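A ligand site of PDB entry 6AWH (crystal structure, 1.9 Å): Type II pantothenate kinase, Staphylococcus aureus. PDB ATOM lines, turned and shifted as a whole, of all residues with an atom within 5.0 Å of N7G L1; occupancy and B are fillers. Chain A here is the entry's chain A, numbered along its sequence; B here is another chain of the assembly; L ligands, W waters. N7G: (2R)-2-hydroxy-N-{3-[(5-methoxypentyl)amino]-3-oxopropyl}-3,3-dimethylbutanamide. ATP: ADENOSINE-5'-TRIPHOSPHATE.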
ATOM      1  N   LYS A 155      -8.037  15.682  30.694  1.00  0.00           N
ATOM      2  CA  LYS A 155      -7.527  14.734  31.680  1.00  0.00           C
ATOM      3  C   LYS A 155      -8.630  14.088  32.454  1.00  0.00           C
ATOM      4  O   LYS A 155      -9.753  14.569  32.512  1.00  0.00           O
ATOM      5  CB  LYS A 155      -6.585  15.431  32.662  1.00  0.00           C
ATOM      6  CG  LYS A 155      -5.266  15.858  32.038  1.00  0.00           C
ATOM      7  CD  LYS A 155      -4.377  16.592  33.039  1.00  0.00           C
ATOM      8  CE  LYS A 155      -3.060  17.032  32.428  1.00  0.00           C
ATOM      9  NZ  LYS A 155      -2.204  15.857  32.110  1.00  0.00           N
ATOM     10  N   VAL A 156      -8.286  12.958  33.065  1.00  0.00           N
ATOM     11  CA  VAL A 156      -9.208  12.195  33.906  1.00  0.00           C
ATOM     12  C   VAL A 156      -9.786  13.094  35.003  1.00  0.00           C
ATOM     13  O   VAL A 156     -11.010  13.064  35.272  1.00  0.00           O
ATOM     14  CB  VAL A 156      -8.547  10.938  34.479  1.00  0.00           C
ATOM     15  CG1 VAL A 156      -9.426  10.222  35.509  1.00  0.00           C
ATOM     16  CG2 VAL A 156      -8.167   9.957  33.359  1.00  0.00           C
ATOM     17  N   ILE A 159     -12.769  15.243  34.098  1.00  0.00           N
ATOM     18  CA  ILE A 159     -14.029  14.492  34.075  1.00  0.00           C
ATOM     19  C   ILE A 159     -14.529  14.218  35.498  1.00  0.00           C
ATOM     20  O   ILE A 159     -15.718  14.424  35.797  1.00  0.00           O
ATOM     21  CB  ILE A 159     -13.911  13.183  33.273  1.00  0.00           C
ATOM     22  CG1 ILE A 159     -13.658  13.526  31.808  1.00  0.00           C
ATOM     23  CG2 ILE A 159     -15.167  12.309  33.449  1.00  0.00           C
ATOM     24  CD1 ILE A 159     -13.475  12.329  30.894  1.00  0.00           C
ATOM     25  N   TYR A 160     -13.634  13.747  36.352  1.00  0.00           N
ATOM     26  CA  TYR A 160     -13.999  13.358  37.753  1.00  0.00           C
ATOM     27  C   TYR A 160     -14.086  14.541  38.761  1.00  0.00           C
ATOM     28  O   TYR A 160     -14.680  14.413  39.832  1.00  0.00           O
ATOM     29  CB  TYR A 160     -13.106  12.223  38.259  1.00  0.00           C
ATOM     30  CG  TYR A 160     -13.715  10.889  37.903  1.00  0.00           C
ATOM     31  CD1 TYR A 160     -13.622  10.387  36.609  1.00  0.00           C
ATOM     32  CD2 TYR A 160     -14.472  10.202  38.819  1.00  0.00           C
ATOM     33  CE1 TYR A 160     -14.224   9.189  36.261  1.00  0.00           C
ATOM     34  CE2 TYR A 160     -15.070   8.984  38.501  1.00  0.00           C
ATOM     35  CZ  TYR A 160     -14.963   8.495  37.214  1.00  0.00           C
ATOM     36  OH  TYR A 160     -15.578   7.318  36.917  1.00  0.00           O
ATOM     37  N   ILE A 167      -8.948   5.654  37.989  1.00  0.00           N
ATOM     38  CA  ILE A 167      -7.573   5.616  37.475  1.00  0.00           C
ATOM     39  C   ILE A 167      -6.928   6.990  37.732  1.00  0.00           C
ATOM     40  O   ILE A 167      -7.632   7.955  37.978  1.00  0.00           O
ATOM     41  CB  ILE A 167      -7.541   5.256  35.978  1.00  0.00           C
ATOM     42  CG1 ILE A 167      -8.349   6.261  35.154  1.00  0.00           C
ATOM     43  CG2 ILE A 167      -8.070   3.838  35.764  1.00  0.00           C
ATOM     44  CD1 ILE A 167      -8.202   6.094  33.655  1.00  0.00           C
ATOM     45  N   ASP A 170      -4.244  12.531  36.528  1.00  0.00           N
ATOM     46  CA  ASP A 170      -3.379  13.235  35.586  1.00  0.00           C
ATOM     47  C   ASP A 170      -3.333  12.617  34.178  1.00  0.00           C
ATOM     48  O   ASP A 170      -2.823  13.235  33.236  1.00  0.00           O
ATOM     49  CB  ASP A 170      -1.948  13.362  36.141  1.00  0.00           C
ATOM     50  CG  ASP A 170      -1.110  14.361  35.354  1.00  0.00           C
ATOM     51  OD1 ASP A 170      -1.536  15.531  35.230  1.00  0.00           O
ATOM     52  OD2 ASP A 170      -0.066  13.967  34.803  1.00  0.00           O
ATOM     53  N   LEU A 171      -3.815  11.400  34.037  1.00  0.00           N
ATOM     54  CA  LEU A 171      -3.867  10.718  32.726  1.00  0.00           C
ATOM     55  C   LEU A 171      -4.714  11.474  31.712  1.00  0.00           C
ATOM     56  O   LEU A 171      -5.701  12.079  32.074  1.00  0.00           O
ATOM     57  CB  LEU A 171      -4.409   9.299  32.859  1.00  0.00           C
ATOM     58  CG  LEU A 171      -3.625   8.259  33.649  1.00  0.00           C
ATOM     59  CD1 LEU A 171      -4.393   6.954  33.668  1.00  0.00           C
ATOM     60  CD2 LEU A 171      -2.238   8.042  33.074  1.00  0.00           C
ATOM     61  N   THR A 172      -4.296  11.464  30.459  1.00  0.00           N
ATOM     62  CA  THR A 172      -5.152  11.936  29.385  1.00  0.00           C
ATOM     63  C   THR A 172      -6.407  11.041  29.314  1.00  0.00           C
ATOM     64  O   THR A 172      -6.299   9.835  29.127  1.00  0.00           O
ATOM     65  CB  THR A 172      -4.445  11.870  28.020  1.00  0.00           C
ATOM     66  OG1 THR A 172      -3.240  12.634  28.080  1.00  0.00           O
ATOM     67  CG2 THR A 172      -5.328  12.433  26.927  1.00  0.00           C
ATOM     68  N   ALA A 173      -7.574  11.655  29.469  1.00  0.00           N
ATOM     69  CA  ALA A 173      -8.869  10.979  29.253  1.00  0.00           C
ATOM     70  C   ALA A 173      -9.295  10.993  27.798  1.00  0.00           C
ATOM     71  O   ALA A 173      -9.832  10.015  27.287  1.00  0.00           O
ATOM     72  CB  ALA A 173      -9.959  11.606  30.093  1.00  0.00           C
ATOM     73  N   GLU A 202       0.996   8.799  22.773  1.00  0.00           N
ATOM     74  CA  GLU A 202       0.176   8.055  23.724  1.00  0.00           C
ATOM     75  C   GLU A 202      -0.365   6.753  23.119  1.00  0.00           C
ATOM     76  O   GLU A 202      -0.469   5.728  23.796  1.00  0.00           O
ATOM     77  CB  GLU A 202      -0.954   8.906  24.282  1.00  0.00           C
ATOM     78  CG  GLU A 202      -0.448  10.009  25.223  1.00  0.00           C
ATOM     79  CD  GLU A 202      -1.536  10.971  25.692  1.00  0.00           C
ATOM     80  OE1 GLU A 202      -2.728  10.780  25.347  1.00  0.00           O
ATOM     81  OE2 GLU A 202      -1.185  11.914  26.445  1.00  0.00           O
ATOM     82  N   THR A 206       0.674   3.159  24.451  1.00  0.00           N
ATOM     83  CA  THR A 206      -0.422   2.296  24.904  1.00  0.00           C
ATOM     84  C   THR A 206      -0.375   0.922  24.230  1.00  0.00           C
ATOM     85  O   THR A 206      -0.516  -0.097  24.885  1.00  0.00           O
ATOM     86  CB  THR A 206      -1.815   2.962  24.683  1.00  0.00           C
ATOM     87  OG1 THR A 206      -1.893   4.137  25.492  1.00  0.00           O
ATOM     88  CG2 THR A 206      -2.945   2.024  25.073  1.00  0.00           C
ATOM     89  N   TYR A 240       5.219   7.968  29.801  1.00  0.00           N
ATOM     90  CA  TYR A 240       4.057   7.082  29.910  1.00  0.00           C
ATOM     91  C   TYR A 240       4.475   5.593  30.003  1.00  0.00           C
ATOM     92  O   TYR A 240       3.867   4.830  30.725  1.00  0.00           O
ATOM     93  CB  TYR A 240       3.000   7.329  28.816  1.00  0.00           C
ATOM     94  CG  TYR A 240       1.731   6.599  29.089  1.00  0.00           C
ATOM     95  CD1 TYR A 240       1.124   6.652  30.347  1.00  0.00           C
ATOM     96  CD2 TYR A 240       1.086   5.842  28.113  1.00  0.00           C
ATOM     97  CE1 TYR A 240      -0.060   5.991  30.637  1.00  0.00           C
ATOM     98  CE2 TYR A 240      -0.106   5.171  28.377  1.00  0.00           C
ATOM     99  CZ  TYR A 240      -0.661   5.244  29.666  1.00  0.00           C
ATOM    100  OH  TYR A 240      -1.845   4.611  29.969  1.00  0.00           O
ATOM    101  N   GLU B  70     -17.912   3.342  37.635  1.00  0.00           N
ATOM    102  CA  GLU B  70     -18.450   3.217  36.264  1.00  0.00           C
ATOM    103  C   GLU B  70     -18.098   1.912  35.551  1.00  0.00           C
ATOM    104  O   GLU B  70     -18.891   1.434  34.751  1.00  0.00           O
ATOM    105  CB  GLU B  70     -18.133   4.448  35.397  1.00  0.00           C
ATOM    106  CG  GLU B  70     -16.688   4.683  35.078  1.00  0.00           C
ATOM    107  CD  GLU B  70     -16.521   5.799  34.051  1.00  0.00           C
ATOM    108  OE1 GLU B  70     -16.667   5.518  32.843  1.00  0.00           O
ATOM    109  OE2 GLU B  70     -16.211   6.938  34.422  1.00  0.00           O
ATOM    110  N   PHE B  71     -16.936   1.345  35.856  1.00  0.00           N
ATOM    111  CA  PHE B  71     -16.485   0.124  35.197  1.00  0.00           C
ATOM    112  C   PHE B  71     -17.342  -1.089  35.558  1.00  0.00           C
ATOM    113  O   PHE B  71     -17.785  -1.864  34.689  1.00  0.00           O
ATOM    114  CB  PHE B  71     -15.023  -0.170  35.486  1.00  0.00           C
ATOM    115  CG  PHE B  71     -14.106   0.967  35.167  1.00  0.00           C
ATOM    116  CD1 PHE B  71     -14.320   1.783  34.041  1.00  0.00           C
ATOM    117  CD2 PHE B  71     -12.995   1.193  35.946  1.00  0.00           C
ATOM    118  CE1 PHE B  71     -13.450   2.822  33.737  1.00  0.00           C
ATOM    119  CE2 PHE B  71     -12.119   2.224  35.643  1.00  0.00           C
ATOM    120  CZ  PHE B  71     -12.348   3.045  34.544  1.00  0.00           C
ATOM    121  N   THR B  99     -16.286   9.696  25.954  1.00  0.00           N
ATOM    122  CA  THR B  99     -15.436  10.893  25.705  1.00  0.00           C
ATOM    123  C   THR B  99     -14.031  10.376  25.450  1.00  0.00           C
ATOM    124  O   THR B  99     -13.357  10.775  24.492  1.00  0.00           O
ATOM    125  CB  THR B  99     -15.500  11.875  26.888  1.00  0.00           C
ATOM    126  OG1 THR B  99     -16.876  12.244  27.113  1.00  0.00           O
ATOM    127  CG2 THR B  99     -14.661  13.122  26.599  1.00  0.00           C
ATOM    128  N   GLY B 100     -13.624   9.487  26.335  1.00  0.00           N
ATOM    129  CA  GLY B 100     -12.467   8.626  26.113  1.00  0.00           C
ATOM    130  C   GLY B 100     -12.881   7.168  26.061  1.00  0.00           C
ATOM    131  O   GLY B 100     -14.038   6.828  26.303  1.00  0.00           O
ATOM    132  N   THR B 101     -11.912   6.306  25.798  1.00  0.00           N
ATOM    133  CA  THR B 101     -12.147   4.902  25.579  1.00  0.00           C
ATOM    134  C   THR B 101     -11.517   4.037  26.668  1.00  0.00           C
ATOM    135  O   THR B 101     -10.326   4.113  26.924  1.00  0.00           O
ATOM    136  CB  THR B 101     -11.664   4.476  24.191  1.00  0.00           C
ATOM    137  OG1 THR B 101     -12.415   5.208  23.194  1.00  0.00           O
ATOM    138  CG2 THR B 101     -11.845   2.957  23.943  1.00  0.00           C
ATOM    139  N   SER B 102     -12.351   3.208  27.275  1.00  0.00           N
ATOM    140  CA  SER B 102     -11.953   2.228  28.294  1.00  0.00           C
ATOM    141  C   SER B 102     -12.216   0.799  27.775  1.00  0.00           C
ATOM    142  O   SER B 102     -13.298   0.493  27.272  1.00  0.00           O
ATOM    143  CB  SER B 102     -12.730   2.522  29.568  1.00  0.00           C
ATOM    144  OG  SER B 102     -12.189   1.846  30.682  1.00  0.00           O
ATOM    145  N   ARG B 113     -10.514  -4.164  33.880  1.00  0.00           N
ATOM    146  CA  ARG B 113     -10.044  -3.143  32.942  1.00  0.00           C
ATOM    147  C   ARG B 113      -8.667  -3.576  32.433  1.00  0.00           C
ATOM    148  O   ARG B 113      -7.746  -3.757  33.204  1.00  0.00           O
ATOM    149  CB  ARG B 113     -10.001  -1.746  33.553  1.00  0.00           C
ATOM    150  CG  ARG B 113      -9.786  -0.615  32.544  1.00  0.00           C
ATOM    151  CD  ARG B 113      -9.936   0.740  33.203  1.00  0.00           C
ATOM    152  NE  ARG B 113      -9.905   1.879  32.283  1.00  0.00           N
ATOM    153  CZ  ARG B 113      -8.817   2.462  31.793  1.00  0.00           C
ATOM    154  NH1 ARG B 113      -7.603   2.013  32.097  1.00  0.00           N
ATOM    155  NH2 ARG B 113      -8.942   3.492  30.966  1.00  0.00           N
ATOM    156  N   GLY B 115      -7.249  -2.031  29.509  1.00  0.00           N
ATOM    157  CA  GLY B 115      -6.654  -0.918  28.804  1.00  0.00           C
ATOM    158  C   GLY B 115      -7.536   0.290  28.671  1.00  0.00           C
ATOM    159  O   GLY B 115      -8.700   0.300  29.071  1.00  0.00           O
ATOM    160  N   GLY B 116      -6.958   1.316  28.078  1.00  0.00           N
ATOM    161  CA  GLY B 116      -7.681   2.522  27.775  1.00  0.00           C
ATOM    162  C   GLY B 116      -6.866   3.428  26.905  1.00  0.00           C
ATOM    163  O   GLY B 116      -5.660   3.224  26.718  1.00  0.00           O
ATOM    164  N   ILE B 117      -7.536   4.393  26.314  1.00  0.00           N
ATOM    165  CA  ILE B 117      -6.915   5.299  25.349  1.00  0.00           C
ATOM    166  C   ILE B 117      -7.755   6.547  25.171  1.00  0.00           C
ATOM    167  O   ILE B 117      -8.976   6.504  25.238  1.00  0.00           O
ATOM    168  CB  ILE B 117      -6.581   4.557  23.999  1.00  0.00           C
ATOM    169  CG1 ILE B 117      -5.729   5.419  23.063  1.00  0.00           C
ATOM    170  CG2 ILE B 117      -7.828   4.057  23.301  1.00  0.00           C
ATOM    171  CD1 ILE B 117      -4.330   5.656  23.577  1.00  0.00           C
ATOM    172  N   GLY B 118      -7.093   7.676  24.947  1.00  0.00           N
ATOM    173  CA  GLY B 118      -7.774   8.956  24.752  1.00  0.00           C
ATOM    174  C   GLY B 118      -8.410   9.190  23.382  1.00  0.00           C
ATOM    175  O   GLY B 118      -8.866  10.277  23.110  1.00  0.00           O
HETATM  176  C06 N7G L   1     -14.098   8.294  32.013  1.00  0.00           C
HETATM  177  C07 N7G L   1     -12.725   7.593  31.809  1.00  0.00           C
HETATM  178  C08 N7G L   1     -12.687   6.325  32.694  1.00  0.00           C
HETATM  179  C09 N7G L   1     -11.606   8.589  32.187  1.00  0.00           C
HETATM  180  C10 N7G L   1     -12.595   7.197  30.318  1.00  0.00           C
HETATM  181  O11 N7G L   1     -12.784   8.411  29.535  1.00  0.00           O
HETATM  182  C12 N7G L   1     -11.246   6.537  29.994  1.00  0.00           C
HETATM  183  O13 N7G L   1     -10.967   5.399  30.360  1.00  0.00           O
HETATM  184  N14 N7G L   1     -10.400   7.295  29.276  1.00  0.00           N
HETATM  185  C15 N7G L   1      -9.038   6.904  28.874  1.00  0.00           C
HETATM  186  C16 N7G L   1      -8.052   7.069  30.027  1.00  0.00           C
HETATM  187  C17 N7G L   1      -6.809   6.308  29.667  1.00  0.00           C
HETATM  188  O18 N7G L   1      -6.809   5.081  29.770  1.00  0.00           O
HETATM  189  N19 N7G L   1      -5.778   6.989  29.181  1.00  0.00           N
HETATM  190  C20 N7G L   1      -4.606   6.231  28.787  1.00  0.00           C
HETATM  191  C21 N7G L   1      -3.514   7.019  28.080  1.00  0.00           C
HETATM  192  C22 N7G L   1      -3.119   8.177  28.948  1.00  0.00           C
HETATM  193  C23 N7G L   1      -1.677   8.611  28.695  1.00  0.00           C
HETATM  194  C24 N7G L   1      -1.270   9.373  29.953  1.00  0.00           C
HETATM  195  O25 N7G L   1      -1.296  10.773  29.767  1.00  0.00           O
HETATM  196  C26 N7G L   1      -0.683  11.484  30.876  1.00  0.00           C
HETATM  197  PG  ATP L   2     -16.736   9.215  29.692  1.00  0.00           P
HETATM  198  O1G ATP L   2     -16.664  10.117  30.909  1.00  0.00           O
HETATM  199  O2G ATP L   2     -15.419   9.056  28.911  1.00  0.00           O
HETATM  200  O3G ATP L   2     -17.383   7.882  30.023  1.00  0.00           O
HETATM  201  PB  ATP L   2     -19.288   9.971  28.472  1.00  0.00           P
HETATM  202  O1B ATP L   2     -19.962  11.366  28.420  1.00  0.00           O
HETATM  203  O2B ATP L   2     -19.904   8.962  29.405  1.00  0.00           O
HETATM  204  O3B ATP L   2     -17.691  10.079  28.686  1.00  0.00           O
HETATM  205  PA  ATP L   2     -20.539   8.766  26.115  1.00  0.00           P
HETATM  206  O1A ATP L   2     -21.889   9.324  26.542  1.00  0.00           O
HETATM  207  O2A ATP L   2     -20.472   7.259  26.035  1.00  0.00           O
HETATM  208  O3A ATP L   2     -19.320   9.428  26.941  1.00  0.00           O
HETATM  209  O5' ATP L   2     -20.080   9.353  24.685  1.00  0.00           O
HETATM  210  C5' ATP L   2     -19.788  10.731  24.475  1.00  0.00           C
HETATM  211  C4' ATP L   2     -19.543  10.925  22.999  1.00  0.00           C
HETATM  212  O4' ATP L   2     -20.750  10.599  22.314  1.00  0.00           O
HETATM  213  C3' ATP L   2     -19.209  12.363  22.609  1.00  0.00           C
HETATM  214  O3' ATP L   2     -17.816  12.674  22.770  1.00  0.00           O
HETATM  215  C2' ATP L   2     -19.635  12.381  21.176  1.00  0.00           C
HETATM  216  O2' ATP L   2     -18.604  11.840  20.369  1.00  0.00           O
HETATM  217  C1' ATP L   2     -20.849  11.425  21.163  1.00  0.00           C
HETATM  218  N9  ATP L   2     -22.197  12.054  21.165  1.00  0.00           N
HETATM  219  C8  ATP L   2     -23.310  11.372  20.797  1.00  0.00           C
HETATM  220  N7  ATP L   2     -24.406  12.157  20.869  1.00  0.00           N
HETATM  221  C5  ATP L   2     -23.993  13.369  21.273  1.00  0.00           C
HETATM  222  C6  ATP L   2     -24.676  14.636  21.553  1.00  0.00           C
HETATM  223  N6  ATP L   2     -26.016  14.724  21.384  1.00  0.00           N
HETATM  224  N1  ATP L   2     -23.915  15.662  21.964  1.00  0.00           N
HETATM  225  C2  ATP L   2     -22.570  15.553  22.132  1.00  0.00           C
HETATM  226  N3  ATP L   2     -21.876  14.415  21.893  1.00  0.00           N
HETATM  227  C4  ATP L   2     -22.533  13.303  21.473  1.00  0.00           C
HETATM  228  O   HOH W   1      -5.233   3.320  30.839  1.00  0.00           O
HETATM  229  O   HOH W   2      -2.789   3.418  27.896  1.00  0.00           O
HETATM  230  O   HOH W   3       0.573  14.340  29.386  1.00  0.00           O
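OG1 of Thr 172 is in hydrogen-bond range of O25 of N7G L1, 3.2 Å away. N of Thr 172 lies within hydrogen-bond range of O25 of N7G L1 (3.2 Å). N of Gly 100 of chain B sits at hydrogen-bond distance from O2G of ATP L2, at 3.2 Å. NH2 of Arg 113 of chain B is in hydrogen-bond range of O13 of N7G L1, 2.8 Å away. The backbone NH of Gly 100 of chain B lies close to an oxygen (O11) of N7G L1 (3.5 Å). The side-chain hydroxyl (OG1) of Thr 99 of chain B sits at hydrogen-bond distance from an oxygen (O3B) of ATP L2, 2.8 Å away. The backbone NH (N) of Thr 99 of chain B is in hydrogen-bond range of an oxygen (O3B) of ATP L2, at 3.1 Å. A nitrogen (N19) of N7G L1 is in hydrogen-bond range of the backbone carbonyl oxygen of Thr 172, at 2.9 Å. The backbone carbonyl oxygen (O) of Ala 173 sits at hydrogen-bond distance from a nitrogen (N14) of N7G L1.
Val 156 touches N7G L1 (CG2 to C09, 3.9 Å). Ile 167 touches N7G L1. Asp 170 touches N7G L1 (O to C26, 3.6 Å). CD2 of Leu 171 touches C24 of N7G L1, 3.5 Å away. Glu 202 touches N7G L1. OH of Tyr 240 touches C20 of N7G L1, 3.4 Å away. Glu 70 of chain B touches N7G L1. Phe 71 of chain B touches N7G L1 (CE1 to C08, 3.7 Å). Thr 101 of chain B touches N7G L1 (O to C15, 3.6 Å). Ser 102 of chain B touches N7G L1 (CB to O13, 3.5 Å). C of Gly 116 of chain B touches O18 of N7G L1, at 3.3 Å. Ile 117 of chain B touches N7G L1. Hydrophobic or aromatic side chains that line N7G L1: Val 156, Ile 167, Leu 171, Tyr 240 and Phe 71 of chain B. 16 residues have an atom within 4 Å of N7G L1: Val 156, Ile 167, Asp 170, Leu 171, Thr 172, Ala 173, Glu 202, Tyr 240, Glu 70 of chain B, Phe 71 of chain B, Gly 100 of chain B, Thr 101 of chain B, Ser 102 of chain B, Arg 113 of chain B, Gly 116 of chain B and Ile 117 of chain B.
Water W1 lies within hydrogen-bond range of an oxygen (O18) of N7G L1 (2.6 Å) and the guanidinium group (NH1) of Arg 113 of chain B (3.0 Å). Water W2 lies within hydrogen-bond range of the side-chain hydroxyl of Tyr 240 (2.6 Å), the side-chain hydroxyl of Thr 206 (2.7 Å) and the backbone carbonyl oxygen of Gly 116 of chain B (3.1 Å).
The side-chain hydroxyl of Tyr 160 is in hydrogen-bond range of the side-chain carboxylate of Glu 70 of chain B (2.6 Å). The guanidinium group of Arg 113 of chain B sits at hydrogen-bond distance from the side-chain hydroxyl of Ser 102 of chain B (2.8 Å). OG1 of Thr 172 lies within hydrogen-bond range of OE2 of Glu 202. OD1 of Asp 170 is in salt-bridge range of NZ of Lys 155 (3.2 Å). O of Thr 101 of chain B sits at hydrogen-bond distance from N of Ile 117 of chain B, at 2.9 Å. The backbone carbonyl oxygen (O) of Leu 171 lies within hydrogen-bond range of the backbone NH (N) of Val 156 (2.9 Å). The backbone carbonyl oxygen of Glu 202 lies within hydrogen-bond range of the side-chain hydroxyl of Thr 206.
O11 of N7G L1 sits at hydrogen-bond distance from O2G of ATP L2.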
